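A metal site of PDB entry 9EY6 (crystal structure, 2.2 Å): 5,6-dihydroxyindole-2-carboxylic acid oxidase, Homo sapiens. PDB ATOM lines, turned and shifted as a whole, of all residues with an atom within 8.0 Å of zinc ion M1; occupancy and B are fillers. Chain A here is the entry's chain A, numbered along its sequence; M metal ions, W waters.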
ATOM      1  N   HIS A 168     -14.582   0.598  25.529  1.00  0.00           N
ATOM      2  CA  HIS A 168     -15.601  -0.339  25.064  1.00  0.00           C
ATOM      3  C   HIS A 168     -16.651   0.400  24.213  1.00  0.00           C
ATOM      4  O   HIS A 168     -17.036  -0.096  23.158  1.00  0.00           O
ATOM      5  CB  HIS A 168     -16.239  -1.099  26.239  1.00  0.00           C
ATOM      6  CG  HIS A 168     -17.111  -2.297  25.913  1.00  0.00           C
ATOM      7  ND1 HIS A 168     -18.460  -2.194  25.667  1.00  0.00           N
ATOM      8  CD2 HIS A 168     -16.843  -3.637  25.849  1.00  0.00           C
ATOM      9  CE1 HIS A 168     -18.981  -3.421  25.504  1.00  0.00           C
ATOM     10  NE2 HIS A 168     -18.008  -4.333  25.554  1.00  0.00           N
ATOM     11  N   TYR A 169     -17.083   1.576  24.654  1.00  0.00           N
ATOM     12  CA  TYR A 169     -18.021   2.408  23.916  1.00  0.00           C
ATOM     13  C   TYR A 169     -17.465   2.754  22.529  1.00  0.00           C
ATOM     14  O   TYR A 169     -18.154   2.572  21.526  1.00  0.00           O
ATOM     15  CB  TYR A 169     -18.341   3.686  24.718  1.00  0.00           C
ATOM     16  CG  TYR A 169     -18.663   4.892  23.844  1.00  0.00           C
ATOM     17  CD1 TYR A 169     -19.917   5.088  23.277  1.00  0.00           C
ATOM     18  CD2 TYR A 169     -17.690   5.832  23.584  1.00  0.00           C
ATOM     19  CE1 TYR A 169     -20.179   6.162  22.432  1.00  0.00           C
ATOM     20  CE2 TYR A 169     -17.912   6.893  22.728  1.00  0.00           C
ATOM     21  CZ  TYR A 169     -19.158   7.069  22.150  1.00  0.00           C
ATOM     22  OH  TYR A 169     -19.277   8.185  21.360  1.00  0.00           O
ATOM     23  N   SER A 171     -15.280   1.335  20.740  1.00  0.00           N
ATOM     24  CA  SER A 171     -15.202   0.173  19.865  1.00  0.00           C
ATOM     25  C   SER A 171     -16.527  -0.234  19.219  1.00  0.00           C
ATOM     26  O   SER A 171     -16.500  -1.012  18.245  1.00  0.00           O
ATOM     27  CB  SER A 171     -14.572  -1.007  20.599  1.00  0.00           C
ATOM     28  OG  SER A 171     -15.454  -1.653  21.497  1.00  0.00           O
ATOM     29  N   VAL A 172     -17.685   0.216  19.758  1.00  0.00           N
ATOM     30  CA  VAL A 172     -18.996  -0.214  19.281  1.00  0.00           C
ATOM     31  C   VAL A 172     -19.800   0.941  18.690  1.00  0.00           C
ATOM     32  O   VAL A 172     -20.864   0.720  18.145  1.00  0.00           O
ATOM     33  CB  VAL A 172     -19.866  -0.978  20.322  1.00  0.00           C
ATOM     34  CG1 VAL A 172     -19.158  -2.171  20.936  1.00  0.00           C
ATOM     35  CG2 VAL A 172     -20.410  -0.082  21.426  1.00  0.00           C
ATOM     36  N   ASP A 188     -18.701  -3.281  14.456  1.00  0.00           N
ATOM     37  CA  ASP A 188     -18.400  -3.515  15.856  1.00  0.00           C
ATOM     38  C   ASP A 188     -16.977  -4.070  15.954  1.00  0.00           C
ATOM     39  O   ASP A 188     -16.743  -5.221  15.595  1.00  0.00           O
ATOM     40  CB  ASP A 188     -19.427  -4.464  16.453  1.00  0.00           C
ATOM     41  CG  ASP A 188     -19.460  -4.572  17.982  1.00  0.00           C
ATOM     42  OD1 ASP A 188     -18.353  -4.617  18.599  1.00  0.00           O
ATOM     43  OD2 ASP A 188     -20.597  -4.647  18.557  1.00  0.00           O
ATOM     44  N   SER A 190     -15.281  -5.101  18.482  1.00  0.00           N
ATOM     45  CA  SER A 190     -14.996  -5.893  19.680  1.00  0.00           C
ATOM     46  C   SER A 190     -16.014  -7.013  19.897  1.00  0.00           C
ATOM     47  O   SER A 190     -15.831  -7.823  20.794  1.00  0.00           O
ATOM     48  CB  SER A 190     -14.939  -5.037  20.873  1.00  0.00           C
ATOM     49  OG  SER A 190     -16.037  -4.116  20.916  1.00  0.00           O
ATOM     50  N   HIS A 191     -17.077  -7.084  19.081  1.00  0.00           N
ATOM     51  CA  HIS A 191     -18.069  -8.146  19.183  1.00  0.00           C
ATOM     52  C   HIS A 191     -18.424  -8.624  17.774  1.00  0.00           C
ATOM     53  O   HIS A 191     -18.153  -7.924  16.791  1.00  0.00           O
ATOM     54  CB  HIS A 191     -19.340  -7.624  19.879  1.00  0.00           C
ATOM     55  CG  HIS A 191     -19.090  -6.872  21.156  1.00  0.00           C
ATOM     56  ND1 HIS A 191     -18.715  -5.546  21.165  1.00  0.00           N
ATOM     57  CD2 HIS A 191     -19.086  -7.267  22.429  1.00  0.00           C
ATOM     58  CE1 HIS A 191     -18.491  -5.175  22.413  1.00  0.00           C
ATOM     59  NE2 HIS A 191     -18.753  -6.199  23.199  1.00  0.00           N
ATOM     60  N   PHE A 196     -13.609 -10.853  19.375  1.00  0.00           N
ATOM     61  CA  PHE A 196     -14.368 -10.746  20.624  1.00  0.00           C
ATOM     62  C   PHE A 196     -13.523 -11.081  21.875  1.00  0.00           C
ATOM     63  O   PHE A 196     -13.410 -10.246  22.792  1.00  0.00           O
ATOM     64  CB  PHE A 196     -15.632 -11.594  20.570  1.00  0.00           C
ATOM     65  CG  PHE A 196     -16.337 -11.783  21.900  1.00  0.00           C
ATOM     66  CD1 PHE A 196     -16.928 -10.720  22.548  1.00  0.00           C
ATOM     67  CD2 PHE A 196     -16.342 -13.013  22.518  1.00  0.00           C
ATOM     68  CE1 PHE A 196     -17.530 -10.903  23.777  1.00  0.00           C
ATOM     69  CE2 PHE A 196     -16.946 -13.188  23.741  1.00  0.00           C
ATOM     70  CZ  PHE A 196     -17.549 -12.137  24.376  1.00  0.00           C
ATOM     71  N   TRP A 199      -9.987  -9.071  22.209  1.00  0.00           N
ATOM     72  CA  TRP A 199     -10.283  -7.688  22.590  1.00  0.00           C
ATOM     73  C   TRP A 199     -10.593  -7.592  24.087  1.00  0.00           C
ATOM     74  O   TRP A 199      -9.987  -6.796  24.815  1.00  0.00           O
ATOM     75  CB  TRP A 199     -11.403  -7.097  21.727  1.00  0.00           C
ATOM     76  CG  TRP A 199     -11.563  -5.600  21.841  1.00  0.00           C
ATOM     77  CD1 TRP A 199     -11.139  -4.689  20.933  1.00  0.00           C
ATOM     78  CD2 TRP A 199     -12.152  -4.827  22.909  1.00  0.00           C
ATOM     79  NE1 TRP A 199     -11.389  -3.414  21.378  1.00  0.00           N
ATOM     80  CE2 TRP A 199     -11.998  -3.473  22.589  1.00  0.00           C
ATOM     81  CE3 TRP A 199     -12.753  -5.158  24.125  1.00  0.00           C
ATOM     82  CZ2 TRP A 199     -12.444  -2.444  23.391  1.00  0.00           C
ATOM     83  CZ3 TRP A 199     -13.230  -4.136  24.926  1.00  0.00           C
ATOM     84  CH2 TRP A 199     -13.061  -2.814  24.577  1.00  0.00           C
ATOM     85  N   HIS A 200     -11.523  -8.413  24.579  1.00  0.00           N
ATOM     86  CA  HIS A 200     -11.967  -8.318  25.972  1.00  0.00           C
ATOM     87  C   HIS A 200     -10.873  -8.771  26.924  1.00  0.00           C
ATOM     88  O   HIS A 200     -10.797  -8.335  28.057  1.00  0.00           O
ATOM     89  CB  HIS A 200     -13.295  -9.078  26.169  1.00  0.00           C
ATOM     90  CG  HIS A 200     -14.486  -8.386  25.574  1.00  0.00           C
ATOM     91  ND1 HIS A 200     -14.759  -8.452  24.224  1.00  0.00           N
ATOM     92  CD2 HIS A 200     -15.458  -7.581  26.121  1.00  0.00           C
ATOM     93  CE1 HIS A 200     -15.860  -7.727  23.972  1.00  0.00           C
ATOM     94  NE2 HIS A 200     -16.319  -7.190  25.099  1.00  0.00           N
ATOM     95  N   HIS A 203      -8.627  -5.700  27.328  1.00  0.00           N
ATOM     96  CA  HIS A 203      -9.434  -4.760  28.099  1.00  0.00           C
ATOM     97  C   HIS A 203      -9.245  -4.986  29.603  1.00  0.00           C
ATOM     98  O   HIS A 203      -8.991  -4.033  30.324  1.00  0.00           O
ATOM     99  CB  HIS A 203     -10.889  -4.999  27.692  1.00  0.00           C
ATOM    100  CG  HIS A 203     -11.818  -3.952  28.080  1.00  0.00           C
ATOM    101  ND1 HIS A 203     -13.122  -4.244  28.457  1.00  0.00           N
ATOM    102  CD2 HIS A 203     -11.695  -2.607  28.107  1.00  0.00           C
ATOM    103  CE1 HIS A 203     -13.746  -3.099  28.700  1.00  0.00           C
ATOM    104  NE2 HIS A 203     -12.893  -2.076  28.512  1.00  0.00           N
ATOM    105  N   GLU A 336     -19.354 -16.580  22.797  1.00  0.00           N
ATOM    106  CA  GLU A 336     -19.918 -15.241  22.762  1.00  0.00           C
ATOM    107  C   GLU A 336     -21.417 -15.351  23.057  1.00  0.00           C
ATOM    108  O   GLU A 336     -22.012 -14.419  23.616  1.00  0.00           O
ATOM    109  CB  GLU A 336     -19.571 -14.534  21.450  1.00  0.00           C
ATOM    110  CG  GLU A 336     -20.033 -13.069  21.375  1.00  0.00           C
ATOM    111  CD  GLU A 336     -19.522 -12.242  20.183  1.00  0.00           C
ATOM    112  OE1 GLU A 336     -18.837 -12.827  19.310  1.00  0.00           O
ATOM    113  OE2 GLU A 336     -19.821 -11.009  20.080  1.00  0.00           O
ATOM    114  N   HIS A 353     -22.045 -15.996  27.260  1.00  0.00           N
ATOM    115  CA  HIS A 353     -21.707 -14.621  27.596  1.00  0.00           C
ATOM    116  C   HIS A 353     -22.897 -13.702  27.388  1.00  0.00           C
ATOM    117  O   HIS A 353     -23.169 -12.849  28.219  1.00  0.00           O
ATOM    118  CB  HIS A 353     -20.397 -14.204  26.914  1.00  0.00           C
ATOM    119  CG  HIS A 353     -20.358 -12.785  26.488  1.00  0.00           C
ATOM    120  ND1 HIS A 353     -20.940 -12.251  25.354  1.00  0.00           N
ATOM    121  CD2 HIS A 353     -19.798 -11.755  27.170  1.00  0.00           C
ATOM    122  CE1 HIS A 353     -20.736 -10.921  25.377  1.00  0.00           C
ATOM    123  NE2 HIS A 353     -20.020 -10.609  26.478  1.00  0.00           N
ATOM    124  N   ASN A 354     -23.585 -13.838  26.246  1.00  0.00           N
ATOM    125  CA  ASN A 354     -24.687 -12.931  25.916  1.00  0.00           C
ATOM    126  C   ASN A 354     -25.862 -13.144  26.888  1.00  0.00           C
ATOM    127  O   ASN A 354     -26.543 -12.191  27.227  1.00  0.00           O
ATOM    128  CB  ASN A 354     -25.178 -13.071  24.485  1.00  0.00           C
ATOM    129  CG  ASN A 354     -24.235 -12.539  23.420  1.00  0.00           C
ATOM    130  OD1 ASN A 354     -23.476 -11.574  23.616  1.00  0.00           O
ATOM    131  ND2 ASN A 354     -24.311 -13.157  22.263  1.00  0.00           N
ATOM    132  N   HIS A 357     -25.145 -11.353  30.244  1.00  0.00           N
ATOM    133  CA  HIS A 357     -25.478  -9.943  30.149  1.00  0.00           C
ATOM    134  C   HIS A 357     -26.987  -9.705  30.187  1.00  0.00           C
ATOM    135  O   HIS A 357     -27.483  -8.777  30.833  1.00  0.00           O
ATOM    136  CB  HIS A 357     -24.944  -9.356  28.834  1.00  0.00           C
ATOM    137  CG  HIS A 357     -23.519  -8.934  28.769  1.00  0.00           C
ATOM    138  ND1 HIS A 357     -23.091  -7.717  29.277  1.00  0.00           N
ATOM    139  CD2 HIS A 357     -22.435  -9.508  28.251  1.00  0.00           C
ATOM    140  CE1 HIS A 357     -21.792  -7.574  29.057  1.00  0.00           C
ATOM    141  NE2 HIS A 357     -21.373  -8.624  28.417  1.00  0.00           N
ATOM    142  N   GLN A 366     -26.911  -3.377  27.726  1.00  0.00           N
ATOM    143  CA  GLN A 366     -26.896  -2.504  26.564  1.00  0.00           C
ATOM    144  C   GLN A 366     -25.438  -2.276  26.132  1.00  0.00           C
ATOM    145  O   GLN A 366     -24.600  -1.869  26.943  1.00  0.00           O
ATOM    146  CB  GLN A 366     -27.584  -1.215  27.014  1.00  0.00           C
ATOM    147  CG  GLN A 366     -28.927  -1.456  27.704  1.00  0.00           C
ATOM    148  CD  GLN A 366     -29.511  -0.209  28.309  1.00  0.00           C
ATOM    149  OE1 GLN A 366     -29.799   0.780  27.625  1.00  0.00           O
ATOM    150  NE2 GLN A 366     -29.723  -0.245  29.622  1.00  0.00           N
ATOM    151  N   THR A 367     -25.150  -2.529  24.852  1.00  0.00           N
ATOM    152  CA  THR A 367     -23.767  -2.789  24.444  1.00  0.00           C
ATOM    153  C   THR A 367     -22.907  -1.543  24.619  1.00  0.00           C
ATOM    154  O   THR A 367     -21.774  -1.656  25.105  1.00  0.00           O
ATOM    155  CB  THR A 367     -23.647  -3.390  23.045  1.00  0.00           C
ATOM    156  OG1 THR A 367     -24.528  -4.516  22.984  1.00  0.00           O
ATOM    157  CG2 THR A 367     -22.228  -3.876  22.782  1.00  0.00           C
ATOM    158  N   HIS A 368     -23.469  -0.340  24.370  1.00  0.00           N
ATOM    159  CA  HIS A 368     -22.694   0.880  24.581  1.00  0.00           C
ATOM    160  C   HIS A 368     -22.496   1.278  26.055  1.00  0.00           C
ATOM    161  O   HIS A 368     -21.626   2.120  26.328  1.00  0.00           O
ATOM    162  CB  HIS A 368     -23.277   2.078  23.825  1.00  0.00           C
ATOM    163  CG  HIS A 368     -24.627   2.456  24.314  1.00  0.00           C
ATOM    164  ND1 HIS A 368     -25.670   1.553  24.237  1.00  0.00           N
ATOM    165  CD2 HIS A 368     -25.106   3.554  24.914  1.00  0.00           C
ATOM    166  CE1 HIS A 368     -26.761   2.111  24.769  1.00  0.00           C
ATOM    167  NE2 HIS A 368     -26.444   3.326  25.183  1.00  0.00           N
ATOM    168  N   SER A 370     -22.526  -1.318  28.880  1.00  0.00           N
ATOM    169  CA  SER A 370     -22.531  -2.439  29.811  1.00  0.00           C
ATOM    170  C   SER A 370     -21.420  -2.384  30.863  1.00  0.00           C
ATOM    171  O   SER A 370     -21.623  -2.885  31.960  1.00  0.00           O
ATOM    172  CB  SER A 370     -22.555  -3.788  29.115  1.00  0.00           C
ATOM    173  OG  SER A 370     -21.661  -3.831  28.036  1.00  0.00           O
ATOM    174  N   PRO A 371     -20.188  -1.924  30.559  1.00  0.00           N
ATOM    175  CA  PRO A 371     -19.134  -1.893  31.575  1.00  0.00           C
ATOM    176  C   PRO A 371     -19.396  -0.939  32.723  1.00  0.00           C
ATOM    177  O   PRO A 371     -18.726  -1.065  33.740  1.00  0.00           O
ATOM    178  CB  PRO A 371     -17.847  -1.531  30.825  1.00  0.00           C
ATOM    179  CG  PRO A 371     -18.213  -1.575  29.373  1.00  0.00           C
ATOM    180  CD  PRO A 371     -19.702  -1.473  29.244  1.00  0.00           C
ATOM    181  N   PHE A 376     -19.777  -6.550  34.882  1.00  0.00           N
ATOM    182  CA  PHE A 376     -19.082  -6.683  33.614  1.00  0.00           C
ATOM    183  C   PHE A 376     -17.667  -7.231  33.825  1.00  0.00           C
ATOM    184  O   PHE A 376     -17.280  -8.154  33.143  1.00  0.00           O
ATOM    185  CB  PHE A 376     -19.021  -5.338  32.883  1.00  0.00           C
ATOM    186  CG  PHE A 376     -18.351  -5.393  31.507  1.00  0.00           C
ATOM    187  CD1 PHE A 376     -16.976  -5.399  31.389  1.00  0.00           C
ATOM    188  CD2 PHE A 376     -19.109  -5.368  30.342  1.00  0.00           C
ATOM    189  CE1 PHE A 376     -16.380  -5.443  30.146  1.00  0.00           C
ATOM    190  CE2 PHE A 376     -18.517  -5.416  29.077  1.00  0.00           C
ATOM    191  CZ  PHE A 376     -17.148  -5.432  28.981  1.00  0.00           C
ATOM    192  N   HIS A 380     -16.659 -10.906  32.376  1.00  0.00           N
ATOM    193  CA  HIS A 380     -15.595 -10.988  31.373  1.00  0.00           C
ATOM    194  C   HIS A 380     -14.373 -11.772  31.855  1.00  0.00           C
ATOM    195  O   HIS A 380     -13.740 -12.411  31.021  1.00  0.00           O
ATOM    196  CB  HIS A 380     -15.303  -9.613  30.729  1.00  0.00           C
ATOM    197  CG  HIS A 380     -16.235  -9.413  29.587  1.00  0.00           C
ATOM    198  ND1 HIS A 380     -15.990 -10.146  28.435  1.00  0.00           N
ATOM    199  CD2 HIS A 380     -17.422  -8.776  29.407  1.00  0.00           C
ATOM    200  CE1 HIS A 380     -16.986  -9.927  27.585  1.00  0.00           C
ATOM    201  NE2 HIS A 380     -17.862  -9.103  28.152  1.00  0.00           N
HETATM  202 ZN    ZN M   1     -18.175  -6.246  25.184  1.00  0.00          ZN
HETATM  203 ZN    ZN M   2     -19.625  -8.778  27.307  1.00  0.00          ZN
HETATM  204  O   HOH W   1     -19.628  -7.413  26.417  1.00  0.00           O
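Merely in contact with zinc ion M1: Phe 376 (3.995 Å). Within 4 Å of zinc ion M1: His 168, His 191, His 200 and Phe 376.
Zinc ion M1 is bound by a ring nitrogen (NE2) of His 168 (2.0 Å), a ring nitrogen (NE2) of His 191 (2.1 Å), a ring nitrogen (NE2) of His 200 (2.1 Å) and water W1 (2.2 Å).
A ring nitrogen (ND1) of His 168 lies close to the backbone carbonyl oxygen (O) of Thr 367. The side-chain hydroxyl (OG) of Ser 171 is in hydrogen-bond range of the backbone carbonyl oxygen (O) of His 168, 2.8 Å away. ND1 of His 191 sits at hydrogen-bond distance from OG of Ser 190 (3.0 Å). ND1 of His 191 lies within hydrogen-bond range of OD1 of Asp 188 (2.8 Å). A ring nitrogen (ND1) of His 200 lies within hydrogen-bond range of the backbone carbonyl oxygen of Phe 196 (2.7 Å).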
